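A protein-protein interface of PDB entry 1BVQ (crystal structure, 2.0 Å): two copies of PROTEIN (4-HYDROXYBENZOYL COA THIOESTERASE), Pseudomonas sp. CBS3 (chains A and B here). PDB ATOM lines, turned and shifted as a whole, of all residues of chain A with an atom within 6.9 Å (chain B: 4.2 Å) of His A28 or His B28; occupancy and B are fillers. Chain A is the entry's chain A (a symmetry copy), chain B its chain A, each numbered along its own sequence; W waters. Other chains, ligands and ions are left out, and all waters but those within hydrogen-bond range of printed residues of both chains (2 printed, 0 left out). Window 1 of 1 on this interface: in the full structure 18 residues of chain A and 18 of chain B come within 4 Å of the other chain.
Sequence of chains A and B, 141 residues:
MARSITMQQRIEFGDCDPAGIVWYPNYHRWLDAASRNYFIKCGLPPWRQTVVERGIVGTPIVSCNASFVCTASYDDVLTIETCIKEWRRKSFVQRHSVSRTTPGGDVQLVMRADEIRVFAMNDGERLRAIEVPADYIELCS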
ATOM      1  N   TRP A  23     -17.250  14.495 -15.526  1.00  0.00           N
ATOM      2  CA  TRP A  23     -18.638  14.692 -15.140  1.00  0.00           C
ATOM      3  C   TRP A  23     -19.433  14.069 -16.296  1.00  0.00           C
ATOM      4  O   TRP A  23     -19.249  14.432 -17.463  1.00  0.00           O
ATOM      5  CB  TRP A  23     -18.877  16.173 -14.964  1.00  0.00           C
ATOM      6  CG  TRP A  23     -20.265  16.446 -14.520  1.00  0.00           C
ATOM      7  CD1 TRP A  23     -20.923  15.753 -13.544  1.00  0.00           C
ATOM      8  CD2 TRP A  23     -21.146  17.485 -14.997  1.00  0.00           C
ATOM      9  NE1 TRP A  23     -22.187  16.302 -13.370  1.00  0.00           N
ATOM     10  CE2 TRP A  23     -22.351  17.366 -14.257  1.00  0.00           C
ATOM     11  CE3 TRP A  23     -21.053  18.465 -16.004  1.00  0.00           C
ATOM     12  CZ2 TRP A  23     -23.448  18.226 -14.505  1.00  0.00           C
ATOM     13  CZ3 TRP A  23     -22.114  19.324 -16.202  1.00  0.00           C
ATOM     14  CH2 TRP A  23     -23.298  19.192 -15.466  1.00  0.00           C
ATOM     15  N   TYR A  24     -20.290  13.120 -15.959  1.00  0.00           N
ATOM     16  CA  TYR A  24     -21.108  12.345 -16.873  1.00  0.00           C
ATOM     17  C   TYR A  24     -21.708  12.971 -18.137  1.00  0.00           C
ATOM     18  O   TYR A  24     -21.547  12.464 -19.275  1.00  0.00           O
ATOM     19  CB  TYR A  24     -21.815  11.167 -16.147  1.00  0.00           C
ATOM     20  CG  TYR A  24     -23.235  11.598 -15.864  1.00  0.00           C
ATOM     21  CD1 TYR A  24     -24.186  11.505 -16.892  1.00  0.00           C
ATOM     22  CD2 TYR A  24     -23.640  12.113 -14.627  1.00  0.00           C
ATOM     23  CE1 TYR A  24     -25.521  11.890 -16.724  1.00  0.00           C
ATOM     24  CE2 TYR A  24     -24.972  12.505 -14.446  1.00  0.00           C
ATOM     25  CZ  TYR A  24     -25.915  12.403 -15.485  1.00  0.00           C
ATOM     26  OH  TYR A  24     -27.256  12.793 -15.329  1.00  0.00           O
ATOM     27  N   PRO A  25     -22.413  14.075 -17.942  1.00  0.00           N
ATOM     28  CA  PRO A  25     -23.039  14.750 -19.063  1.00  0.00           C
ATOM     29  C   PRO A  25     -22.083  15.060 -20.162  1.00  0.00           C
ATOM     30  O   PRO A  25     -22.493  15.211 -21.312  1.00  0.00           O
ATOM     31  CB  PRO A  25     -23.820  15.974 -18.543  1.00  0.00           C
ATOM     32  CG  PRO A  25     -24.042  15.704 -17.059  1.00  0.00           C
ATOM     33  CD  PRO A  25     -22.966  14.645 -16.661  1.00  0.00           C
ATOM     34  N   ASN A  26     -20.792  15.152 -19.805  1.00  0.00           N
ATOM     35  CA  ASN A  26     -19.767  15.446 -20.807  1.00  0.00           C
ATOM     36  C   ASN A  26     -19.629  14.308 -21.759  1.00  0.00           C
ATOM     37  O   ASN A  26     -19.365  14.529 -22.937  1.00  0.00           O
ATOM     38  CB  ASN A  26     -18.374  15.927 -20.322  1.00  0.00           C
ATOM     39  CG  ASN A  26     -18.452  17.223 -19.531  1.00  0.00           C
ATOM     40  OD1 ASN A  26     -19.149  18.190 -19.916  1.00  0.00           O
ATOM     41  ND2 ASN A  26     -17.747  17.247 -18.412  1.00  0.00           N
ATOM     42  N   TYR A  27     -19.809  13.074 -21.268  1.00  0.00           N
ATOM     43  CA  TYR A  27     -19.667  12.018 -22.235  1.00  0.00           C
ATOM     44  C   TYR A  27     -20.691  12.186 -23.378  1.00  0.00           C
ATOM     45  O   TYR A  27     -20.372  11.874 -24.516  1.00  0.00           O
ATOM     46  CB  TYR A  27     -19.849  10.646 -21.669  1.00  0.00           C
ATOM     47  CG  TYR A  27     -18.722  10.225 -20.778  1.00  0.00           C
ATOM     48  CD1 TYR A  27     -17.476   9.835 -21.270  1.00  0.00           C
ATOM     49  CD2 TYR A  27     -18.941  10.188 -19.400  1.00  0.00           C
ATOM     50  CE1 TYR A  27     -16.448   9.430 -20.399  1.00  0.00           C
ATOM     51  CE2 TYR A  27     -17.946   9.782 -18.509  1.00  0.00           C
ATOM     52  CZ  TYR A  27     -16.705   9.388 -19.020  1.00  0.00           C
ATOM     53  OH  TYR A  27     -15.737   8.994 -18.117  1.00  0.00           O
ATOM     54  N   HIS A  28     -21.910  12.676 -23.081  1.00  0.00           N
ATOM     55  CA  HIS A  28     -22.934  12.843 -24.135  1.00  0.00           C
ATOM     56  C   HIS A  28     -22.553  13.868 -25.178  1.00  0.00           C
ATOM     57  O   HIS A  28     -22.962  13.805 -26.323  1.00  0.00           O
ATOM     58  CB  HIS A  28     -24.296  13.099 -23.536  1.00  0.00           C
ATOM     59  CG  HIS A  28     -24.688  11.919 -22.719  1.00  0.00           C
ATOM     60  ND1 HIS A  28     -25.081  10.759 -23.337  1.00  0.00           N
ATOM     61  CD2 HIS A  28     -24.723  11.704 -21.351  1.00  0.00           C
ATOM     62  CE1 HIS A  28     -25.347   9.871 -22.344  1.00  0.00           C
ATOM     63  NE2 HIS A  28     -25.143  10.394 -21.137  1.00  0.00           N
ATOM     64  N   ARG A  29     -21.734  14.824 -24.756  1.00  0.00           N
ATOM     65  CA  ARG A  29     -21.255  15.881 -25.608  1.00  0.00           C
ATOM     66  C   ARG A  29     -20.325  15.305 -26.643  1.00  0.00           C
ATOM     67  O   ARG A  29     -20.361  15.645 -27.838  1.00  0.00           O
ATOM     68  CB  ARG A  29     -20.469  17.024 -24.848  1.00  0.00           C
ATOM     69  CG  ARG A  29     -21.278  18.037 -23.977  1.00  0.00           C
ATOM     70  CD  ARG A  29     -20.624  19.464 -23.774  1.00  0.00           C
ATOM     71  NE  ARG A  29     -19.261  19.409 -23.237  1.00  0.00           N
ATOM     72  CZ  ARG A  29     -18.099  19.183 -23.883  1.00  0.00           C
ATOM     73  NH1 ARG A  29     -18.063  18.987 -25.202  1.00  0.00           N
ATOM     74  NH2 ARG A  29     -16.936  19.169 -23.169  1.00  0.00           N
ATOM     75  N   TRP A  30     -19.482  14.426 -26.172  1.00  0.00           N
ATOM     76  CA  TRP A  30     -18.510  13.786 -27.026  1.00  0.00           C
ATOM     77  C   TRP A  30     -19.147  12.729 -27.930  1.00  0.00           C
ATOM     78  O   TRP A  30     -18.702  12.489 -29.046  1.00  0.00           O
ATOM     79  CB  TRP A  30     -17.402  13.114 -26.112  1.00  0.00           C
ATOM     80  CG  TRP A  30     -16.699  14.152 -25.316  1.00  0.00           C
ATOM     81  CD1 TRP A  30     -16.430  15.417 -25.791  1.00  0.00           C
ATOM     82  CD2 TRP A  30     -16.163  14.099 -23.960  1.00  0.00           C
ATOM     83  NE1 TRP A  30     -15.775  16.173 -24.818  1.00  0.00           N
ATOM     84  CE2 TRP A  30     -15.605  15.400 -23.690  1.00  0.00           C
ATOM     85  CE3 TRP A  30     -16.106  13.117 -22.956  1.00  0.00           C
ATOM     86  CZ2 TRP A  30     -15.020  15.727 -22.462  1.00  0.00           C
ATOM     87  CZ3 TRP A  30     -15.519  13.445 -21.729  1.00  0.00           C
ATOM     88  CH2 TRP A  30     -14.987  14.731 -21.499  1.00  0.00           C
ATOM     89  N   LEU A  31     -20.203  12.081 -27.463  1.00  0.00           N
ATOM     90  CA  LEU A  31     -20.794  11.083 -28.325  1.00  0.00           C
ATOM     91  C   LEU A  31     -21.550  11.805 -29.434  1.00  0.00           C
ATOM     92  O   LEU A  31     -21.658  11.285 -30.557  1.00  0.00           O
ATOM     93  CB  LEU A  31     -21.813  10.150 -27.616  1.00  0.00           C
ATOM     94  CG  LEU A  31     -21.260   9.228 -26.508  1.00  0.00           C
ATOM     95  CD1 LEU A  31     -22.349   8.364 -25.812  1.00  0.00           C
ATOM     96  CD2 LEU A  31     -20.189   8.402 -27.116  1.00  0.00           C
ATOM     97  N   ASP A  32     -22.100  12.987 -29.091  1.00  0.00           N
ATOM     98  CA  ASP A  32     -22.844  13.797 -30.067  1.00  0.00           C
ATOM     99  C   ASP A  32     -21.898  14.168 -31.207  1.00  0.00           C
ATOM    100  O   ASP A  32     -22.184  14.095 -32.396  1.00  0.00           O
ATOM    101  CB  ASP A  32     -23.410  15.112 -29.431  1.00  0.00           C
ATOM    102  CG  ASP A  32     -24.387  15.759 -30.461  1.00  0.00           C
ATOM    103  OD1 ASP A  32     -25.217  14.942 -31.045  1.00  0.00           O
ATOM    104  OD2 ASP A  32     -24.411  16.916 -30.762  1.00  0.00           O
ATOM    105  N   ALA A  33     -20.700  14.574 -30.821  1.00  0.00           N
ATOM    106  CA  ALA A  33     -19.675  14.948 -31.758  1.00  0.00           C
ATOM    107  C   ALA A  33     -19.276  13.713 -32.551  1.00  0.00           C
ATOM    108  O   ALA A  33     -19.109  13.751 -33.771  1.00  0.00           O
ATOM    109  CB  ALA A  33     -18.469  15.525 -31.009  1.00  0.00           C
ATOM    110  N   ALA A  34     -19.140  12.596 -31.847  1.00  0.00           N
ATOM    111  CA  ALA A  34     -18.763  11.361 -32.481  1.00  0.00           C
ATOM    112  C   ALA A  34     -19.768  10.894 -33.519  1.00  0.00           C
ATOM    113  O   ALA A  34     -19.425  10.356 -34.575  1.00  0.00           O
ATOM    114  CB  ALA A  34     -18.518  10.287 -31.436  1.00  0.00           C
ATOM    115  N   CYS A  64     -31.702   6.119 -26.037  1.00  0.00           N
ATOM    116  CA  CYS A  64     -30.331   5.770 -25.881  1.00  0.00           C
ATOM    117  C   CYS A  64     -30.105   4.927 -24.634  1.00  0.00           C
ATOM    118  O   CYS A  64     -30.809   5.020 -23.656  1.00  0.00           O
ATOM    119  CB  CYS A  64     -29.552   7.036 -25.934  1.00  0.00           C
ATOM    120  SG  CYS A  64     -30.068   8.011 -24.523  1.00  0.00           S
ATOM    121  N   ALA A  66     -26.848   3.584 -22.188  1.00  0.00           N
ATOM    122  CA  ALA A  66     -25.428   3.669 -21.876  1.00  0.00           C
ATOM    123  C   ALA A  66     -25.092   2.941 -20.583  1.00  0.00           C
ATOM    124  O   ALA A  66     -25.901   2.862 -19.674  1.00  0.00           O
ATOM    125  CB  ALA A  66     -25.035   5.106 -21.603  1.00  0.00           C
ATOM    126  N   PHE A  68     -21.667   2.665 -17.931  1.00  0.00           N
ATOM    127  CA  PHE A  68     -20.324   3.188 -17.620  1.00  0.00           C
ATOM    128  C   PHE A  68     -19.662   2.145 -16.769  1.00  0.00           C
ATOM    129  O   PHE A  68     -20.187   1.714 -15.725  1.00  0.00           O
ATOM    130  CB  PHE A  68     -20.398   4.549 -16.892  1.00  0.00           C
ATOM    131  CG  PHE A  68     -21.315   5.578 -17.583  1.00  0.00           C
ATOM    132  CD1 PHE A  68     -22.703   5.485 -17.437  1.00  0.00           C
ATOM    133  CD2 PHE A  68     -20.774   6.620 -18.361  1.00  0.00           C
ATOM    134  CE1 PHE A  68     -23.551   6.416 -18.052  1.00  0.00           C
ATOM    135  CE2 PHE A  68     -21.628   7.552 -18.979  1.00  0.00           C
ATOM    136  CZ  PHE A  68     -23.015   7.448 -18.821  1.00  0.00           C
ATOM    137  N   MET A 111     -16.884   3.274 -21.458  1.00  0.00           N
ATOM    138  CA  MET A 111     -18.314   3.302 -21.600  1.00  0.00           C
ATOM    139  C   MET A 111     -18.767   2.747 -22.932  1.00  0.00           C
ATOM    140  O   MET A 111     -18.008   2.681 -23.907  1.00  0.00           O
ATOM    141  CB  MET A 111     -18.755   4.771 -21.460  1.00  0.00           C
ATOM    142  CG  MET A 111     -20.141   5.026 -21.930  1.00  0.00           C
ATOM    143  SD  MET A 111     -20.143   6.675 -22.619  1.00  0.00           S
ATOM    144  CE  MET A 111     -21.753   7.089 -21.950  1.00  0.00           C
ATOM    145  N   ALA A 113     -22.456   2.770 -25.378  1.00  0.00           N
ATOM    146  CA  ALA A 113     -23.760   3.400 -25.491  1.00  0.00           C
ATOM    147  C   ALA A 113     -24.374   3.164 -26.854  1.00  0.00           C
ATOM    148  O   ALA A 113     -23.701   3.134 -27.877  1.00  0.00           O
ATOM    149  CB  ALA A 113     -23.635   4.918 -25.347  1.00  0.00           C
ATOM    150  N   GLU A 115     -27.232   4.678 -29.263  1.00  0.00           N
ATOM    151  CA  GLU A 115     -28.068   5.827 -29.490  1.00  0.00           C
ATOM    152  C   GLU A 115     -28.989   5.606 -30.671  1.00  0.00           C
ATOM    153  O   GLU A 115     -28.539   5.339 -31.765  1.00  0.00           O
ATOM    154  CB  GLU A 115     -27.218   7.033 -29.898  1.00  0.00           C
ATOM    155  CG  GLU A 115     -26.271   7.557 -28.778  1.00  0.00           C
ATOM    156  CD  GLU A 115     -25.675   8.838 -29.242  1.00  0.00           C
ATOM    157  OE1 GLU A 115     -25.233   9.003 -30.346  1.00  0.00           O
ATOM    158  OE2 GLU A 115     -25.697   9.751 -28.344  1.00  0.00           O
ATOM    159  N   ARG A 117     -31.202   7.235 -33.240  1.00  0.00           N
ATOM    160  CA  ARG A 117     -31.432   8.538 -33.850  1.00  0.00           C
ATOM    161  C   ARG A 117     -32.216   8.469 -35.153  1.00  0.00           C
ATOM    162  O   ARG A 117     -32.451   7.399 -35.698  1.00  0.00           O
ATOM    163  CB  ARG A 117     -30.104   9.048 -34.219  1.00  0.00           C
ATOM    164  CG  ARG A 117     -29.318   9.486 -32.980  1.00  0.00           C
ATOM    165  CD  ARG A 117     -27.956   9.851 -33.469  1.00  0.00           C
ATOM    166  NE  ARG A 117     -27.066  10.328 -32.417  1.00  0.00           N
ATOM    167  CZ  ARG A 117     -26.942  11.591 -32.015  1.00  0.00           C
ATOM    168  NH1 ARG A 117     -27.656  12.582 -32.542  1.00  0.00           N
ATOM    169  NH2 ARG A 117     -26.049  11.886 -31.036  1.00  0.00           N
ATOM    170  N   TYR B  24     -29.388  17.936 -26.656  1.00  0.00           N
ATOM    171  CA  TYR B  24     -29.497  16.741 -25.841  1.00  0.00           C
ATOM    172  C   TYR B  24     -28.682  16.573 -24.553  1.00  0.00           C
ATOM    173  O   TYR B  24     -29.218  16.282 -23.456  1.00  0.00           O
ATOM    174  CB  TYR B  24     -29.924  15.510 -26.687  1.00  0.00           C
ATOM    175  CG  TYR B  24     -28.675  14.715 -26.988  1.00  0.00           C
ATOM    176  CD1 TYR B  24     -28.179  13.840 -26.008  1.00  0.00           C
ATOM    177  CD2 TYR B  24     -27.973  14.831 -28.194  1.00  0.00           C
ATOM    178  CE1 TYR B  24     -27.024  13.072 -26.196  1.00  0.00           C
ATOM    179  CE2 TYR B  24     -26.814  14.070 -28.393  1.00  0.00           C
ATOM    180  CZ  TYR B  24     -26.331  13.196 -27.403  1.00  0.00           C
ATOM    181  OH  TYR B  24     -25.169  12.426 -27.578  1.00  0.00           O
ATOM    182  N   PRO B  25     -27.375  16.748 -24.684  1.00  0.00           N
ATOM    183  CA  PRO B  25     -26.500  16.602 -23.537  1.00  0.00           C
ATOM    184  C   PRO B  25     -26.915  17.443 -22.380  1.00  0.00           C
ATOM    185  O   PRO B  25     -26.581  17.130 -21.239  1.00  0.00           O
ATOM    186  CB  PRO B  25     -25.040  16.821 -23.985  1.00  0.00           C
ATOM    187  CG  PRO B  25     -25.050  16.600 -25.493  1.00  0.00           C
ATOM    188  CD  PRO B  25     -26.535  16.789 -25.935  1.00  0.00           C
ATOM    189  N   ASN B  26     -27.654  18.524 -22.678  1.00  0.00           N
ATOM    190  CA  ASN B  26     -28.121  19.416 -21.617  1.00  0.00           C
ATOM    191  C   ASN B  26     -29.121  18.723 -20.756  1.00  0.00           C
ATOM    192  O   ASN B  26     -29.165  18.970 -19.555  1.00  0.00           O
ATOM    193  CB  ASN B  26     -28.622  20.832 -22.007  1.00  0.00           C
ATOM    194  CG  ASN B  26     -27.545  21.660 -22.691  1.00  0.00           C
ATOM    195  OD1 ASN B  26     -26.372  21.705 -22.255  1.00  0.00           O
ATOM    196  ND2 ASN B  26     -27.934  22.308 -23.776  1.00  0.00           N
ATOM    197  N   TYR B  27     -29.936  17.842 -21.353  1.00  0.00           N
ATOM    198  CA  TYR B  27     -30.875  17.202 -20.471  1.00  0.00           C
ATOM    199  C   TYR B  27     -30.137  16.428 -19.359  1.00  0.00           C
ATOM    200  O   TYR B  27     -30.623  16.382 -18.239  1.00  0.00           O
ATOM    201  CB  TYR B  27     -31.792  16.238 -21.155  1.00  0.00           C
ATOM    202  CG  TYR B  27     -32.801  16.911 -22.033  1.00  0.00           C
ATOM    203  CD1 TYR B  27     -33.915  17.581 -21.527  1.00  0.00           C
ATOM    204  CD2 TYR B  27     -32.637  16.832 -23.417  1.00  0.00           C
ATOM    205  CE1 TYR B  27     -34.848  18.186 -22.388  1.00  0.00           C
ATOM    206  CE2 TYR B  27     -33.549  17.413 -24.299  1.00  0.00           C
ATOM    207  CZ  TYR B  27     -34.664  18.075 -23.775  1.00  0.00           C
ATOM    208  OH  TYR B  27     -35.550  18.642 -24.669  1.00  0.00           O
ATOM    209  N   HIS B  28     -28.970  15.826 -19.662  1.00  0.00           N
ATOM    210  CA  HIS B  28     -28.228  15.059 -18.638  1.00  0.00           C
ATOM    211  C   HIS B  28     -27.724  15.916 -17.500  1.00  0.00           C
ATOM    212  O   HIS B  28     -27.555  15.467 -16.381  1.00  0.00           O
ATOM    213  CB  HIS B  28     -27.139  14.223 -19.266  1.00  0.00           C
ATOM    214  CG  HIS B  28     -27.765  13.240 -20.191  1.00  0.00           C
ATOM    215  ND1 HIS B  28     -28.429  12.151 -19.686  1.00  0.00           N
ATOM    216  CD2 HIS B  28     -27.855  13.188 -21.572  1.00  0.00           C
ATOM    217  CE1 HIS B  28     -28.904  11.465 -20.757  1.00  0.00           C
ATOM    218  NE2 HIS B  28     -28.586  12.052 -21.909  1.00  0.00           N
ATOM    219  N   ARG B  29     -27.496  17.187 -17.811  1.00  0.00           N
ATOM    220  CA  ARG B  29     -27.022  18.155 -16.857  1.00  0.00           C
ATOM    221  C   ARG B  29     -28.098  18.420 -15.838  1.00  0.00           C
ATOM    222  O   ARG B  29     -27.860  18.510 -14.621  1.00  0.00           O
ATOM    223  CB  ARG B  29     -26.615  19.546 -17.490  1.00  0.00           C
ATOM    224  CG  ARG B  29     -25.287  19.638 -18.306  1.00  0.00           C
ATOM    225  CD  ARG B  29     -24.599  21.063 -18.366  1.00  0.00           C
ATOM    226  NE  ARG B  29     -25.491  22.119 -18.852  1.00  0.00           N
ATOM    227  CZ  ARG B  29     -26.431  22.817 -18.183  1.00  0.00           C
ATOM    228  NH1 ARG B  29     -26.656  22.613 -16.884  1.00  0.00           N
ATOM    229  NH2 ARG B  29     -27.157  23.760 -18.851  1.00  0.00           N
ATOM    230  N   TRP B  30     -29.294  18.549 -16.347  1.00  0.00           N
ATOM    231  CA  TRP B  30     -30.440  18.820 -15.511  1.00  0.00           C
ATOM    232  C   TRP B  30     -30.880  17.586 -14.722  1.00  0.00           C
ATOM    233  O   TRP B  30     -31.391  17.685 -13.613  1.00  0.00           O
ATOM    234  CB  TRP B  30     -31.628  19.322 -16.434  1.00  0.00           C
ATOM    235  CG  TRP B  30     -31.248  20.585 -17.114  1.00  0.00           C
ATOM    236  CD1 TRP B  30     -30.466  21.555 -16.527  1.00  0.00           C
ATOM    237  CD2 TRP B  30     -31.579  21.074 -18.448  1.00  0.00           C
ATOM    238  NE1 TRP B  30     -30.265  22.618 -17.409  1.00  0.00           N
ATOM    239  CE2 TRP B  30     -30.924  22.351 -18.589  1.00  0.00           C
ATOM    240  CE3 TRP B  30     -32.332  20.578 -19.526  1.00  0.00           C
ATOM    241  CZ2 TRP B  30     -30.999  23.109 -19.763  1.00  0.00           C
ATOM    242  CZ3 TRP B  30     -32.407  21.338 -20.699  1.00  0.00           C
ATOM    243  CH2 TRP B  30     -31.748  22.581 -20.802  1.00  0.00           C
ATOM    244  N   LEU B  31     -30.686  16.403 -15.280  1.00  0.00           N
ATOM    245  CA  LEU B  31     -31.109  15.244 -14.526  1.00  0.00           C
ATOM    246  C   LEU B  31     -30.114  15.030 -13.392  1.00  0.00           C
ATOM    247  O   LEU B  31     -30.489  14.525 -12.320  1.00  0.00           O
ATOM    248  CB  LEU B  31     -31.149  13.927 -15.348  1.00  0.00           C
ATOM    249  CG  LEU B  31     -32.168  13.858 -16.506  1.00  0.00           C
ATOM    250  CD1 LEU B  31     -32.110  12.530 -17.312  1.00  0.00           C
ATOM    251  CD2 LEU B  31     -33.510  14.107 -15.927  1.00  0.00           C
ATOM    252  N   ASP B  32     -28.842  15.385 -13.658  1.00  0.00           N
ATOM    253  CA  ASP B  32     -27.781  15.247 -12.649  1.00  0.00           C
ATOM    254  C   ASP B  32     -28.144  16.116 -11.446  1.00  0.00           C
ATOM    255  O   ASP B  32     -28.063  15.752 -10.279  1.00  0.00           O
ATOM    256  CB  ASP B  32     -26.384  15.698 -13.196  1.00  0.00           C
ATOM    257  CG  ASP B  32     -25.304  15.273 -12.155  1.00  0.00           C
ATOM    258  OD1 ASP B  32     -25.425  14.069 -11.672  1.00  0.00           O
ATOM    259  OD2 ASP B  32     -24.410  15.963 -11.761  1.00  0.00           O
HETATM  260  O   HOH W   1     -28.649  10.366 -17.277  1.00  0.00           O
HETATM  261  O   HOH W   2     -26.220   9.655 -25.890  1.00  0.00           O
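The side-chain hydroxyl (OH) of Tyr B24 is in hydrogen-bond range of the backbone carbonyl oxygen (O) of His A28 (2.9 Å).
The side-chain hydroxyl of Tyr B24 lies within hydrogen-bond range of the backbone NH of Asp A32.
OE2 of Glu A115 lies within hydrogen-bond range of OH of Tyr B24 (2.8 Å).
OH of Tyr A24 sits at hydrogen-bond distance from O of His B28.
NE1 of Trp A23 lies within hydrogen-bond range of OD2 of Asp B32 (2.8 Å).
N of Asp B32 sits at hydrogen-bond distance from OH of Tyr A24 (3.5 Å).
The side-chain amide nitrogen of Asn A26 lies within hydrogen-bond range of the backbone carbonyl oxygen of Trp A23, 3.3 Å away.
OD1 of Asp A32 is in salt-bridge range of NH2 of Arg A117.
NE of Arg A117 is in salt-bridge range of OE1 of Glu A115.
Among the printed residues, merely in contact across the chains: His A28 with His B28 (3.5 Å), Trp A23 with Arg B29 (3.5 Å), Arg A117 with Tyr B24 (3.5 Å), Pro A25 with His B28 (3.6 Å), His A28 with Pro B25 (3.6 Å), Arg A29 with Pro B25 (3.8 Å) and Pro A25 with Arg B29 (3.8 Å).
Of the printed residues of chain B, Trp A23 touches Arg B29 and Asp B32.
Printed residues of chain B within 4 Å of Tyr A24: His B28 (2.9 Å) and Asp B32 (3.2 Å).
His A28 touches just these residues of chain B: Tyr B24 (2.9 Å), Pro B25 (3.6 Å) and His B28 (3.5 Å).
Of the printed residues of chain B, Arg A29 touches Pro B25 (3.8 Å).
Of the printed residues of chain B, Glu A115 touches Tyr B24 (2.8 Å).
Of the printed residues of chain A, Tyr B24 touches His A28 (2.9 Å), Asp A32 (3.2 Å), Glu A115 (2.8 Å) and Arg A117 (3.5 Å).
Of chain A, only Tyr A24 (2.9 Å), Pro A25 (3.6 Å) and His A28 (3.5 Å) come within 4 Å of His B28.
The nearest printed residue of chain B that does not touch His A28 is Asn B26 (6.4 Å).
The nearest residue of chain A that does not touch His B28 is Cys A64 (5.0 Å).
Of the 19 printed residues of chain A, 8 touch a printed residue of chain B.
Hydrophobic or aromatic side chains of chain A that line the printed part of chain B: Trp A23, Tyr A24, Pro A25 and His A28.
Of the 9 printed residues of chain B, 5 touch a printed residue of chain A.
Hydrophobic or aromatic side chains of chain B within 4 Å of the printed part of chain A: Tyr B24, Pro B25 and His B28.
Among the printed residues, no Asp or Glu carboxylate lies within 4 Å of a Lys or Arg side-chain nitrogen of the other chain.
Tyr A24 touches His B28, and with the chains exchanged His A28 touches Tyr B24.
Tyr A24 touches Asp B32, and with the chains exchanged Asp A32 touches Tyr B24.
Pro A25 touches His B28, and with the chains exchanged His A28 touches Pro B25.
His A28 touches its own counterpart, His B28.
Positions printed for both chains: 24, 25, 26, 27, 28, 29, 30, 31 and 32.
Of the 13 pairs that touch across the chains among the printed residues, 9 have their exchanged pair printed and touching as well.
Water W2 lies within hydrogen-bond range of OE2 of Glu A115 (2.5 Å), ND1 of His A28 (3.0 Å) and OH of Tyr B24 (3.4 Å).
Water W1 lies within hydrogen-bond range of ND1 of His B28 and OH of Tyr A24.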
